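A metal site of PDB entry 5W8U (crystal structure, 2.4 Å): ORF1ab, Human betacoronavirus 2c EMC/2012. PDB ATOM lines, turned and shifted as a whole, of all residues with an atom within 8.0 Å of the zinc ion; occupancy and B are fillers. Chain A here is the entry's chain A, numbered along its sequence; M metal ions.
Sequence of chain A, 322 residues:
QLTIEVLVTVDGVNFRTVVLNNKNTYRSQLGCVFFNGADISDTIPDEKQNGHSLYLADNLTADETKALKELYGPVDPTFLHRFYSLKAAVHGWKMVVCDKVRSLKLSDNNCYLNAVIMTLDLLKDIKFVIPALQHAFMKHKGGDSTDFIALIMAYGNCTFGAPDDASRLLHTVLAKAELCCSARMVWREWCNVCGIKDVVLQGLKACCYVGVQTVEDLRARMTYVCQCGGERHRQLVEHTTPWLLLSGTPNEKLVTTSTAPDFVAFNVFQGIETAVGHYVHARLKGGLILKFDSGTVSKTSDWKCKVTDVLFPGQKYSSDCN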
ATOM      1  N   TRP A 190      17.264 -29.989  28.364  1.00  0.00           N
ATOM      2  CA  TRP A 190      18.102 -30.833  27.520  1.00  0.00           C
ATOM      3  C   TRP A 190      18.159 -30.273  26.106  1.00  0.00           C
ATOM      4  O   TRP A 190      17.240 -29.593  25.645  1.00  0.00           O
ATOM      5  CB  TRP A 190      17.619 -32.293  27.514  1.00  0.00           C
ATOM      6  CG  TRP A 190      16.269 -32.562  26.919  1.00  0.00           C
ATOM      7  CD1 TRP A 190      16.004 -32.979  25.639  1.00  0.00           C
ATOM      8  CD2 TRP A 190      14.997 -32.479  27.579  1.00  0.00           C
ATOM      9  NE1 TRP A 190      14.641 -33.137  25.459  1.00  0.00           N
ATOM     10  CE2 TRP A 190      14.005 -32.839  26.632  1.00  0.00           C
ATOM     11  CE3 TRP A 190      14.601 -32.118  28.877  1.00  0.00           C
ATOM     12  CZ2 TRP A 190      12.651 -32.854  26.959  1.00  0.00           C
ATOM     13  CZ3 TRP A 190      13.256 -32.131  29.183  1.00  0.00           C
ATOM     14  CH2 TRP A 190      12.291 -32.504  28.223  1.00  0.00           C
ATOM     15  N   CYS A 191      19.274 -30.563  25.442  1.00  0.00           N
ATOM     16  CA  CYS A 191      19.537 -30.203  24.060  1.00  0.00           C
ATOM     17  C   CYS A 191      20.313 -31.351  23.433  1.00  0.00           C
ATOM     18  O   CYS A 191      21.286 -31.826  24.037  1.00  0.00           O
ATOM     19  CB  CYS A 191      20.333 -28.892  23.976  1.00  0.00           C
ATOM     20  SG  CYS A 191      21.293 -28.633  22.474  1.00  0.00           S
ATOM     21  N   ASN A 192      19.881 -31.801  22.254  1.00  0.00           N
ATOM     22  CA  ASN A 192      20.458 -33.011  21.671  1.00  0.00           C
ATOM     23  C   ASN A 192      21.952 -32.880  21.411  1.00  0.00           C
ATOM     24  O   ASN A 192      22.630 -33.914  21.264  1.00  0.00           O
ATOM     25  CB  ASN A 192      19.736 -33.368  20.372  1.00  0.00           C
ATOM     26  CG  ASN A 192      18.323 -33.878  20.615  1.00  0.00           C
ATOM     27  OD1 ASN A 192      18.027 -34.399  21.684  1.00  0.00           O
ATOM     28  ND2 ASN A 192      17.465 -33.733  19.611  1.00  0.00           N
ATOM     29  N   VAL A 193      22.483 -31.671  21.348  1.00  0.00           N
ATOM     30  CA  VAL A 193      23.913 -31.453  21.146  1.00  0.00           C
ATOM     31  C   VAL A 193      24.624 -31.146  22.449  1.00  0.00           C
ATOM     32  O   VAL A 193      25.732 -31.636  22.691  1.00  0.00           O
ATOM     33  CB  VAL A 193      24.135 -30.333  20.112  1.00  0.00           C
ATOM     34  CG1 VAL A 193      25.610 -30.253  19.717  1.00  0.00           C
ATOM     35  CG2 VAL A 193      23.276 -30.568  18.877  1.00  0.00           C
ATOM     36  N   CYS A 194      24.003 -30.333  23.316  1.00  0.00           N
ATOM     37  CA  CYS A 194      24.655 -29.865  24.534  1.00  0.00           C
ATOM     38  C   CYS A 194      24.509 -30.840  25.707  1.00  0.00           C
ATOM     39  O   CYS A 194      25.359 -30.828  26.600  1.00  0.00           O
ATOM     40  CB  CYS A 194      24.089 -28.497  24.940  1.00  0.00           C
ATOM     41  SG  CYS A 194      24.360 -27.211  23.717  1.00  0.00           S
ATOM     42  N   GLY A 195      23.469 -31.652  25.729  1.00  0.00           N
ATOM     43  CA  GLY A 195      23.243 -32.594  26.801  1.00  0.00           C
ATOM     44  C   GLY A 195      22.077 -32.180  27.684  1.00  0.00           C
ATOM     45  O   GLY A 195      21.250 -31.328  27.323  1.00  0.00           O
ATOM     46  N   TYR A 224      12.687 -23.807  22.997  1.00  0.00           N
ATOM     47  CA  TYR A 224      13.209 -22.476  22.711  1.00  0.00           C
ATOM     48  C   TYR A 224      14.653 -22.644  22.256  1.00  0.00           C
ATOM     49  O   TYR A 224      15.254 -23.706  22.426  1.00  0.00           O
ATOM     50  CB  TYR A 224      13.087 -21.550  23.929  1.00  0.00           C
ATOM     51  CG  TYR A 224      13.722 -22.118  25.181  1.00  0.00           C
ATOM     52  CD1 TYR A 224      14.982 -21.714  25.602  1.00  0.00           C
ATOM     53  CD2 TYR A 224      13.055 -23.069  25.946  1.00  0.00           C
ATOM     54  CE1 TYR A 224      15.561 -22.239  26.740  1.00  0.00           C
ATOM     55  CE2 TYR A 224      13.624 -23.603  27.090  1.00  0.00           C
ATOM     56  CZ  TYR A 224      14.875 -23.182  27.484  1.00  0.00           C
ATOM     57  OH  TYR A 224      15.437 -23.720  28.623  1.00  0.00           O
ATOM     58  N   VAL A 225      15.212 -21.576  21.683  1.00  0.00           N
ATOM     59  CA  VAL A 225      16.531 -21.659  21.079  1.00  0.00           C
ATOM     60  C   VAL A 225      17.593 -21.876  22.152  1.00  0.00           C
ATOM     61  O   VAL A 225      17.551 -21.268  23.235  1.00  0.00           O
ATOM     62  CB  VAL A 225      16.815 -20.410  20.230  1.00  0.00           C
ATOM     63  CG1 VAL A 225      16.986 -19.160  21.091  1.00  0.00           C
ATOM     64  CG2 VAL A 225      18.040 -20.630  19.337  1.00  0.00           C
ATOM     65  N   CYS A 226      18.522 -22.775  21.872  1.00  0.00           N
ATOM     66  CA  CYS A 226      19.652 -23.065  22.734  1.00  0.00           C
ATOM     67  C   CYS A 226      20.835 -22.164  22.395  1.00  0.00           C
ATOM     68  O   CYS A 226      20.901 -21.565  21.326  1.00  0.00           O
ATOM     69  CB  CYS A 226      20.060 -24.541  22.597  1.00  0.00           C
ATOM     70  SG  CYS A 226      21.215 -25.090  23.853  1.00  0.00           S
ATOM     71  N   GLN A 227      21.791 -22.089  23.330  1.00  0.00           N
ATOM     72  CA  GLN A 227      22.977 -21.267  23.099  1.00  0.00           C
ATOM     73  C   GLN A 227      23.772 -21.762  21.895  1.00  0.00           C
ATOM     74  O   GLN A 227      24.481 -20.975  21.256  1.00  0.00           O
ATOM     75  CB  GLN A 227      23.862 -21.228  24.347  1.00  0.00           C
ATOM     76  CG  GLN A 227      24.836 -20.062  24.367  1.00  0.00           C
ATOM     77  CD  GLN A 227      25.685 -19.982  25.642  1.00  0.00           C
ATOM     78  OE1 GLN A 227      25.212 -20.291  26.735  1.00  0.00           O
ATOM     79  NE2 GLN A 227      26.931 -19.571  25.499  1.00  0.00           N
ATOM     80  N   CYS A 228      23.663 -23.046  21.558  1.00  0.00           N
ATOM     81  CA  CYS A 228      24.318 -23.605  20.385  1.00  0.00           C
ATOM     82  C   CYS A 228      23.571 -23.313  19.090  1.00  0.00           C
ATOM     83  O   CYS A 228      24.083 -23.650  18.011  1.00  0.00           O
ATOM     84  CB  CYS A 228      24.481 -25.119  20.540  1.00  0.00           C
ATOM     85  SG  CYS A 228      22.930 -26.056  20.478  1.00  0.00           S
ATOM     86  N   GLY A 229      22.389 -22.714  19.158  1.00  0.00           N
ATOM     87  CA  GLY A 229      21.572 -22.507  17.976  1.00  0.00           C
ATOM     88  C   GLY A 229      20.501 -23.552  17.739  1.00  0.00           C
ATOM     89  O   GLY A 229      19.590 -23.303  16.931  1.00  0.00           O
ATOM     90  N   GLY A 230      20.579 -24.703  18.397  1.00  0.00           N
ATOM     91  CA  GLY A 230      19.575 -25.741  18.268  1.00  0.00           C
ATOM     92  C   GLY A 230      18.329 -25.448  19.070  1.00  0.00           C
ATOM     93  O   GLY A 230      18.085 -24.314  19.513  1.00  0.00           O
ATOM     94  N   GLU A 231      17.532 -26.478  19.272  1.00  0.00           N
ATOM     95  CA  GLU A 231      16.317 -26.337  20.055  1.00  0.00           C
ATOM     96  C   GLU A 231      16.539 -26.994  21.413  1.00  0.00           C
ATOM     97  O   GLU A 231      16.955 -28.158  21.493  1.00  0.00           O
ATOM     98  CB  GLU A 231      15.114 -26.924  19.315  1.00  0.00           C
ATOM     99  CG  GLU A 231      14.532 -25.854  18.380  1.00  0.00           C
ATOM    100  CD  GLU A 231      13.132 -26.044  17.853  1.00  0.00           C
ATOM    101  OE1 GLU A 231      12.474 -25.014  17.528  1.00  0.00           O
ATOM    102  OE2 GLU A 231      12.688 -27.230  17.760  1.00  0.00           O
ATOM    103  N   ARG A 232      16.326 -26.224  22.459  1.00  0.00           N
ATOM    104  CA  ARG A 232      16.456 -26.679  23.828  1.00  0.00           C
ATOM    105  C   ARG A 232      15.070 -26.923  24.405  1.00  0.00           C
ATOM    106  O   ARG A 232      14.100 -26.245  24.049  1.00  0.00           O
ATOM    107  CB  ARG A 232      17.210 -25.653  24.665  1.00  0.00           C
ATOM    108  CG  ARG A 232      17.469 -26.102  26.095  1.00  0.00           C
ATOM    109  CD  ARG A 232      18.606 -25.296  26.723  1.00  0.00           C
ATOM    110  NE  ARG A 232      18.396 -23.862  26.551  1.00  0.00           N
ATOM    111  CZ  ARG A 232      19.277 -22.923  26.892  1.00  0.00           C
ATOM    112  NH1 ARG A 232      20.449 -23.273  27.429  1.00  0.00           N
ATOM    113  NH2 ARG A 232      18.996 -21.641  26.705  1.00  0.00           N
ATOM    114  N   HIS A 233      14.976 -27.910  25.281  1.00  0.00           N
ATOM    115  CA  HIS A 233      13.735 -28.259  25.932  1.00  0.00           C
ATOM    116  C   HIS A 233      13.875 -28.106  27.436  1.00  0.00           C
ATOM    117  O   HIS A 233      14.974 -28.205  27.992  1.00  0.00           O
ATOM    118  CB  HIS A 233      13.312 -29.679  25.577  1.00  0.00           C
ATOM    119  CG  HIS A 233      13.318 -29.947  24.107  1.00  0.00           C
ATOM    120  ND1 HIS A 233      12.252 -29.650  23.284  1.00  0.00           N
ATOM    121  CD2 HIS A 233      14.280 -30.465  23.302  1.00  0.00           C
ATOM    122  CE1 HIS A 233      12.549 -29.989  22.037  1.00  0.00           C
ATOM    123  NE2 HIS A 233      13.773 -30.484  22.020  1.00  0.00           N
HETATM  124 ZN    ZN M   1      22.380 -26.703  22.596  1.00  0.00          ZN
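The backbone NH (N) of Val 193 lies close to the side-chain sulfur (SG) of Cys 191 (3.5 Å). The side-chain sulfur (SG) of Cys 228 lies close to the backbone NH (N) of Gly 230 (3.4 Å).
Of the 16 residues printed, 4 come within 4 Å of the zinc ion. The nearest printed residue that does not touch the zinc ion is Gln 227 (4.7 Å).
The zinc ion is bound by SG of Cys 191 (2.2 Å), SG of Cys 228 (2.3 Å), SG of Cys 194 (2.3 Å) and SG of Cys 226 (2.4 Å). The zinc ion has four donor atoms within binding distance.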
